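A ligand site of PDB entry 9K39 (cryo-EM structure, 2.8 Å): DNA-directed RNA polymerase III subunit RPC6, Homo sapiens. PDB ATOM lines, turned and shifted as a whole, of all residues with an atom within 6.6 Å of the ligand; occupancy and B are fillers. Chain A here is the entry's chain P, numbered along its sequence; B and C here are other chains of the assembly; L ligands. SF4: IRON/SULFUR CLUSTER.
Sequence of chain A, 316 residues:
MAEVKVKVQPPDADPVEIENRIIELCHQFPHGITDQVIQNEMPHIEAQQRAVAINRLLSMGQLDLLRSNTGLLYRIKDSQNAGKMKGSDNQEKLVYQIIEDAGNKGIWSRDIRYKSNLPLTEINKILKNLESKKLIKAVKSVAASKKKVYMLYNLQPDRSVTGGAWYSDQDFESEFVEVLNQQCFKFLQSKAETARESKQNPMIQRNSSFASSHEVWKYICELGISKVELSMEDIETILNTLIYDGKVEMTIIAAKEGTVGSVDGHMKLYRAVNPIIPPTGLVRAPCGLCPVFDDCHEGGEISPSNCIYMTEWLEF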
ATOM      1  N   PRO A 286       9.302 -17.392  -2.005  1.00  0.00           N
ATOM      2  CA  PRO A 286       9.917 -16.296  -1.231  1.00  0.00           C
ATOM      3  C   PRO A 286      11.353 -16.027  -1.603  1.00  0.00           C
ATOM      4  O   PRO A 286      11.841 -14.903  -1.394  1.00  0.00           O
ATOM      5  CB  PRO A 286       9.794 -16.792   0.217  1.00  0.00           C
ATOM      6  CG  PRO A 286       8.686 -17.790   0.201  1.00  0.00           C
ATOM      7  CD  PRO A 286       8.768 -18.457  -1.143  1.00  0.00           C
ATOM      8  N   CYS A 287      12.064 -17.016  -2.161  1.00  0.00           N
ATOM      9  CA  CYS A 287      13.465 -16.818  -2.514  1.00  0.00           C
ATOM     10  C   CYS A 287      13.623 -15.829  -3.668  1.00  0.00           C
ATOM     11  O   CYS A 287      14.620 -15.118  -3.735  1.00  0.00           O
ATOM     12  CB  CYS A 287      14.100 -18.158  -2.884  1.00  0.00           C
ATOM     13  SG  CYS A 287      13.622 -19.535  -1.814  1.00  0.00           S
ATOM     14  N   GLY A 288      12.643 -15.787  -4.575  1.00  0.00           N
ATOM     15  CA  GLY A 288      12.733 -14.894  -5.722  1.00  0.00           C
ATOM     16  C   GLY A 288      12.492 -13.430  -5.398  1.00  0.00           C
ATOM     17  O   GLY A 288      12.950 -12.559  -6.148  1.00  0.00           O
ATOM     18  N   CYS A 290      13.269 -12.145  -2.259  1.00  0.00           N
ATOM     19  CA  CYS A 290      14.019 -11.844  -1.055  1.00  0.00           C
ATOM     20  C   CYS A 290      14.970 -10.679  -1.298  1.00  0.00           C
ATOM     21  O   CYS A 290      15.671 -10.652  -2.310  1.00  0.00           O
ATOM     22  CB  CYS A 290      14.800 -13.069  -0.597  1.00  0.00           C
ATOM     23  SG  CYS A 290      15.803 -12.786   0.874  1.00  0.00           S
ATOM     24  N   PRO A 291      15.028  -9.694  -0.387  1.00  0.00           N
ATOM     25  CA  PRO A 291      15.987  -8.599  -0.553  1.00  0.00           C
ATOM     26  C   PRO A 291      17.384  -8.911  -0.049  1.00  0.00           C
ATOM     27  O   PRO A 291      18.324  -8.195  -0.412  1.00  0.00           O
ATOM     28  CB  PRO A 291      15.356  -7.458   0.260  1.00  0.00           C
ATOM     29  CG  PRO A 291      14.618  -8.170   1.349  1.00  0.00           C
ATOM     30  CD  PRO A 291      14.124  -9.466   0.749  1.00  0.00           C
ATOM     31  N   VAL A 292      17.553  -9.953   0.768  1.00  0.00           N
ATOM     32  CA  VAL A 292      18.853 -10.325   1.306  1.00  0.00           C
ATOM     33  C   VAL A 292      19.262 -11.651   0.682  1.00  0.00           C
ATOM     34  O   VAL A 292      20.010 -12.442   1.283  1.00  0.00           O
ATOM     35  CB  VAL A 292      18.806 -10.374   2.849  1.00  0.00           C
ATOM     36  CG1 VAL A 292      17.992 -11.574   3.357  1.00  0.00           C
ATOM     37  CG2 VAL A 292      20.208 -10.328   3.449  1.00  0.00           C
ATOM     38  N   PHE A 293      18.776 -11.898  -0.544  1.00  0.00           N
ATOM     39  CA  PHE A 293      19.065 -13.141  -1.248  1.00  0.00           C
ATOM     40  C   PHE A 293      20.558 -13.377  -1.412  1.00  0.00           C
ATOM     41  O   PHE A 293      21.009 -14.529  -1.462  1.00  0.00           O
ATOM     42  CB  PHE A 293      18.358 -13.128  -2.599  1.00  0.00           C
ATOM     43  CG  PHE A 293      18.829 -14.193  -3.546  1.00  0.00           C
ATOM     44  CD1 PHE A 293      18.372 -15.493  -3.433  1.00  0.00           C
ATOM     45  CD2 PHE A 293      19.713 -13.889  -4.577  1.00  0.00           C
ATOM     46  CE1 PHE A 293      18.789 -16.472  -4.311  1.00  0.00           C
ATOM     47  CE2 PHE A 293      20.139 -14.866  -5.458  1.00  0.00           C
ATOM     48  CZ  PHE A 293      19.679 -16.161  -5.322  1.00  0.00           C
ATOM     49  N   ASP A 294      21.352 -12.305  -1.509  1.00  0.00           N
ATOM     50  CA  ASP A 294      22.796 -12.472  -1.712  1.00  0.00           C
ATOM     51  C   ASP A 294      23.464 -13.095  -0.492  1.00  0.00           C
ATOM     52  O   ASP A 294      24.402 -13.877  -0.627  1.00  0.00           O
ATOM     53  CB  ASP A 294      23.432 -11.120  -2.048  1.00  0.00           C
ATOM     54  CG  ASP A 294      22.953 -10.562  -3.372  1.00  0.00           C
ATOM     55  OD1 ASP A 294      22.610 -11.365  -4.266  1.00  0.00           O
ATOM     56  OD2 ASP A 294      22.921  -9.319  -3.522  1.00  0.00           O
ATOM     57  N   ASP A 295      22.986 -12.764   0.708  1.00  0.00           N
ATOM     58  CA  ASP A 295      23.574 -13.277   1.940  1.00  0.00           C
ATOM     59  C   ASP A 295      23.067 -14.659   2.317  1.00  0.00           C
ATOM     60  O   ASP A 295      23.332 -15.120   3.431  1.00  0.00           O
ATOM     61  CB  ASP A 295      23.303 -12.304   3.095  1.00  0.00           C
ATOM     62  CG  ASP A 295      23.888 -10.923   2.840  1.00  0.00           C
ATOM     63  OD1 ASP A 295      24.834 -10.824   2.026  1.00  0.00           O
ATOM     64  OD2 ASP A 295      23.419  -9.948   3.457  1.00  0.00           O
ATOM     65  N   CYS A 296      22.337 -15.337   1.430  1.00  0.00           N
ATOM     66  CA  CYS A 296      21.835 -16.674   1.724  1.00  0.00           C
ATOM     67  C   CYS A 296      22.982 -17.672   1.758  1.00  0.00           C
ATOM     68  O   CYS A 296      23.876 -17.649   0.915  1.00  0.00           O
ATOM     69  CB  CYS A 296      20.801 -17.094   0.690  1.00  0.00           C
ATOM     70  SG  CYS A 296      20.321 -18.841   0.793  1.00  0.00           S
ATOM     71  N   HIS A 297      22.943 -18.573   2.750  1.00  0.00           N
ATOM     72  CA  HIS A 297      23.947 -19.621   2.873  1.00  0.00           C
ATOM     73  C   HIS A 297      23.348 -20.792   3.626  1.00  0.00           C
ATOM     74  O   HIS A 297      22.366 -20.652   4.365  1.00  0.00           O
ATOM     75  CB  HIS A 297      25.212 -19.110   3.581  1.00  0.00           C
ATOM     76  CG  HIS A 297      26.353 -20.075   3.558  1.00  0.00           C
ATOM     77  ND1 HIS A 297      26.814 -20.656   2.400  1.00  0.00           N
ATOM     78  CD2 HIS A 297      27.122 -20.570   4.557  1.00  0.00           C
ATOM     79  CE1 HIS A 297      27.814 -21.468   2.679  1.00  0.00           C
ATOM     80  NE2 HIS A 297      28.033 -21.430   3.989  1.00  0.00           N
ATOM     81  N   ILE A 302      21.601 -16.519   8.201  1.00  0.00           N
ATOM     82  CA  ILE A 302      20.541 -16.503   7.210  1.00  0.00           C
ATOM     83  C   ILE A 302      20.579 -17.842   6.484  1.00  0.00           C
ATOM     84  O   ILE A 302      21.392 -18.047   5.579  1.00  0.00           O
ATOM     85  CB  ILE A 302      20.686 -15.323   6.228  1.00  0.00           C
ATOM     86  CG1 ILE A 302      20.695 -14.002   6.989  1.00  0.00           C
ATOM     87  CG2 ILE A 302      19.555 -15.335   5.209  1.00  0.00           C
ATOM     88  CD1 ILE A 302      20.870 -12.784   6.103  1.00  0.00           C
ATOM     89  N   SER A 303      19.712 -18.760   6.894  1.00  0.00           N
ATOM     90  CA  SER A 303      19.650 -20.094   6.334  1.00  0.00           C
ATOM     91  C   SER A 303      18.227 -20.409   5.905  1.00  0.00           C
ATOM     92  O   SER A 303      17.270 -19.932   6.519  1.00  0.00           O
ATOM     93  CB  SER A 303      20.129 -21.146   7.343  1.00  0.00           C
ATOM     94  OG  SER A 303      20.051 -22.448   6.814  1.00  0.00           O
ATOM     95  N   PRO A 304      18.048 -21.203   4.844  1.00  0.00           N
ATOM     96  CA  PRO A 304      16.694 -21.597   4.446  1.00  0.00           C
ATOM     97  C   PRO A 304      15.973 -22.412   5.502  1.00  0.00           C
ATOM     98  O   PRO A 304      14.733 -22.408   5.538  1.00  0.00           O
ATOM     99  CB  PRO A 304      16.921 -22.407   3.163  1.00  0.00           C
ATOM    100  CG  PRO A 304      18.357 -22.830   3.224  1.00  0.00           C
ATOM    101  CD  PRO A 304      19.064 -21.706   3.911  1.00  0.00           C
ATOM    102  N   SER A 305      16.699 -23.109   6.379  1.00  0.00           N
ATOM    103  CA  SER A 305      16.050 -23.897   7.409  1.00  0.00           C
ATOM    104  C   SER A 305      15.321 -23.010   8.423  1.00  0.00           C
ATOM    105  O   SER A 305      14.194 -23.311   8.828  1.00  0.00           O
ATOM    106  CB  SER A 305      17.081 -24.781   8.118  1.00  0.00           C
ATOM    107  OG  SER A 305      18.118 -23.995   8.690  1.00  0.00           O
ATOM    108  N   ASN A 306      15.949 -21.907   8.828  1.00  0.00           N
ATOM    109  CA  ASN A 306      15.370 -20.987   9.794  1.00  0.00           C
ATOM    110  C   ASN A 306      14.906 -19.680   9.153  1.00  0.00           C
ATOM    111  O   ASN A 306      14.962 -18.628   9.795  1.00  0.00           O
ATOM    112  CB  ASN A 306      16.358 -20.712  10.930  1.00  0.00           C
ATOM    113  CG  ASN A 306      17.731 -20.288  10.430  1.00  0.00           C
ATOM    114  OD1 ASN A 306      17.872 -19.800   9.316  1.00  0.00           O
ATOM    115  ND2 ASN A 306      18.744 -20.484  11.265  1.00  0.00           N
ATOM    116  N   CYS A 307      14.470 -19.724   7.894  1.00  0.00           N
ATOM    117  CA  CYS A 307      14.021 -18.526   7.212  1.00  0.00           C
ATOM    118  C   CYS A 307      12.683 -18.052   7.758  1.00  0.00           C
ATOM    119  O   CYS A 307      11.800 -18.862   8.058  1.00  0.00           O
ATOM    120  CB  CYS A 307      13.909 -18.781   5.708  1.00  0.00           C
ATOM    121  SG  CYS A 307      13.198 -17.417   4.776  1.00  0.00           S
ATOM    122  N   ILE A 308      12.526 -16.732   7.893  1.00  0.00           N
ATOM    123  CA  ILE A 308      11.260 -16.169   8.356  1.00  0.00           C
ATOM    124  C   ILE A 308      10.306 -15.977   7.180  1.00  0.00           C
ATOM    125  O   ILE A 308       9.081 -16.139   7.326  1.00  0.00           O
ATOM    126  CB  ILE A 308      11.509 -14.857   9.117  1.00  0.00           C
ATOM    127  CG1 ILE A 308      12.488 -15.078  10.258  1.00  0.00           C
ATOM    128  CG2 ILE A 308      10.197 -14.284   9.634  1.00  0.00           C
ATOM    129  CD1 ILE A 308      12.017 -16.085  11.288  1.00  0.00           C
ATOM    130  N   TYR A 309      10.839 -15.643   6.002  1.00  0.00           N
ATOM    131  CA  TYR A 309      10.001 -15.435   4.829  1.00  0.00           C
ATOM    132  C   TYR A 309       9.244 -16.704   4.466  1.00  0.00           C
ATOM    133  O   TYR A 309       8.016 -16.697   4.332  1.00  0.00           O
ATOM    134  CB  TYR A 309      10.844 -14.972   3.645  1.00  0.00           C
ATOM    135  CG  TYR A 309      11.595 -13.685   3.883  1.00  0.00           C
ATOM    136  CD1 TYR A 309      10.995 -12.452   3.683  1.00  0.00           C
ATOM    137  CD2 TYR A 309      12.928 -13.704   4.295  1.00  0.00           C
ATOM    138  CE1 TYR A 309      11.683 -11.280   3.902  1.00  0.00           C
ATOM    139  CE2 TYR A 309      13.626 -12.530   4.511  1.00  0.00           C
ATOM    140  CZ  TYR A 309      12.998 -11.323   4.312  1.00  0.00           C
ATOM    141  OH  TYR A 309      13.685 -10.157   4.524  1.00  0.00           O
ATOM    142  N   MET A 310       9.965 -17.823   4.315  1.00  0.00           N
ATOM    143  CA  MET A 310       9.307 -19.081   3.990  1.00  0.00           C
ATOM    144  C   MET A 310       8.416 -19.568   5.123  1.00  0.00           C
ATOM    145  O   MET A 310       7.396 -20.209   4.869  1.00  0.00           O
ATOM    146  CB  MET A 310      10.350 -20.136   3.630  1.00  0.00           C
ATOM    147  CG  MET A 310      11.019 -19.890   2.284  1.00  0.00           C
ATOM    148  SD  MET A 310      12.096 -21.240   1.762  1.00  0.00           S
ATOM    149  CE  MET A 310      13.379 -21.141   2.999  1.00  0.00           C
ATOM    150  N   PHE B  38      16.582  -9.826   8.830  1.00  0.00           N
ATOM    151  CA  PHE B  38      15.621 -10.037   7.739  1.00  0.00           C
ATOM    152  C   PHE B  38      14.748  -8.792   7.627  1.00  0.00           C
ATOM    153  O   PHE B  38      13.714  -8.676   8.302  1.00  0.00           O
ATOM    154  CB  PHE B  38      14.779 -11.282   8.006  1.00  0.00           C
ATOM    155  CG  PHE B  38      15.570 -12.561   8.057  1.00  0.00           C
ATOM    156  CD1 PHE B  38      16.100 -13.007   9.253  1.00  0.00           C
ATOM    157  CD2 PHE B  38      15.782 -13.307   6.910  1.00  0.00           C
ATOM    158  CE1 PHE B  38      16.834 -14.180   9.315  1.00  0.00           C
ATOM    159  CE2 PHE B  38      16.511 -14.479   6.959  1.00  0.00           C
ATOM    160  CZ  PHE B  38      17.043 -14.918   8.162  1.00  0.00           C
ATOM    161  N   ASN C 445      17.223 -23.713  -2.237  1.00  0.00           N
ATOM    162  CA  ASN C 445      16.791 -23.339  -0.895  1.00  0.00           C
ATOM    163  C   ASN C 445      15.459 -23.980  -0.532  1.00  0.00           C
ATOM    164  O   ASN C 445      15.251 -24.374   0.620  1.00  0.00           O
ATOM    165  CB  ASN C 445      16.713 -21.813  -0.773  1.00  0.00           C
ATOM    166  CG  ASN C 445      18.057 -21.144  -0.943  1.00  0.00           C
ATOM    167  OD1 ASN C 445      19.103 -21.719  -0.604  1.00  0.00           O
ATOM    168  ND2 ASN C 445      18.057 -19.921  -1.452  1.00  0.00           N
ATOM    169  N   ARG C 449      14.902 -26.434   2.596  1.00  0.00           N
ATOM    170  CA  ARG C 449      13.878 -26.212   3.611  1.00  0.00           C
ATOM    171  C   ARG C 449      12.979 -27.426   3.765  1.00  0.00           C
ATOM    172  O   ARG C 449      12.601 -27.797   4.876  1.00  0.00           O
ATOM    173  CB  ARG C 449      13.060 -24.967   3.267  1.00  0.00           C
ATOM    174  CG  ARG C 449      11.935 -24.669   4.248  1.00  0.00           C
ATOM    175  CD  ARG C 449      12.458 -24.535   5.666  1.00  0.00           C
ATOM    176  NE  ARG C 449      11.408 -24.143   6.600  1.00  0.00           N
ATOM    177  CZ  ARG C 449      11.114 -22.888   6.921  1.00  0.00           C
ATOM    178  NH1 ARG C 449      11.799 -21.889   6.378  1.00  0.00           N
ATOM    179  NH2 ARG C 449      10.143 -22.615   7.782  1.00  0.00           N
HETATM  180 FE1  SF4 L   1      14.894 -15.263   2.251  1.00  0.00          FE
HETATM  181 FE2  SF4 L   1      17.273 -16.603   2.479  1.00  0.00          FE
HETATM  182 FE3  SF4 L   1      15.260 -17.635   0.935  1.00  0.00          FE
HETATM  183 FE4  SF4 L   1      15.021 -17.605   3.658  1.00  0.00          FE
HETATM  184  S1  SF4 L   1      16.551 -18.764   2.437  1.00  0.00           S
HETATM  185  S2  SF4 L   1      13.426 -17.011   2.136  1.00  0.00           S
HETATM  186  S3  SF4 L   1      16.069 -15.650   4.166  1.00  0.00           S
HETATM  187  S4  SF4 L   1      16.391 -15.689   0.580  1.00  0.00           S
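The backbone nitrogen (N) of Pro 304 lies close to a sulfur (S1) of the ligand.
SG of Cys 287 touches FE3 of the ligand, at 3.7 Å.
CB of Cys 296 touches FE2 of the ligand, at 3.99 Å.
Ile 302 touches the ligand.
CD2 of Tyr 309 touches FE1 of the ligand (3.2 Å).
Met 310 touches the ligand (CG to S2, 3.8 Å).
Phe 38 of chain B touches the ligand (CE2 to S3, 3.1 Å).
Hydrophobic or aromatic side chains that line the ligand: Ile 302, Pro 304, Tyr 309, Met 310 and Phe 38 of chain B.
Within 4 Å of the ligand: Cys 287, Cys 290, Cys 296, Ile 302, Pro 304, Cys 307, Tyr 309, Met 310 and Phe 38 of chain B.
The nearest printed residue that does not touch the ligand is Pro 286 (4.1 Å).
SG of Cys 307 binds FE4 of the ligand.
The side-chain sulfur (SG) of Cys 290 lies close to a sulfur (S4) of the ligand (3.0 Å).
SG of Cys 307 lies close to N of Tyr 309, at 3.2 Å.
SG of Cys 307 lies close to N of Met 310, 3.3 Å away.
O of Cys 307 is in hydrogen-bond range of NH1 of Arg 449 of chain C (3.5 Å).
The side-chain sulfur (SG) of Cys 290 is in hydrogen-bond range of the backbone NH (N) of Phe 293, 3.4 Å away.
The side-chain sulfur of Cys 290 sits at hydrogen-bond distance from the backbone NH of Val 292, 3.3 Å away.
O of Pro 304 is in hydrogen-bond range of NH1 of Arg 449 of chain C (3.1 Å).
The backbone carbonyl oxygen (O) of Ile 302 sits at hydrogen-bond distance from the backbone NH (N) of His 297 (3.3 Å).
SG of Cys 296 is in hydrogen-bond range of ND2 of Asn 445 of chain C, 3.4 Å away.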
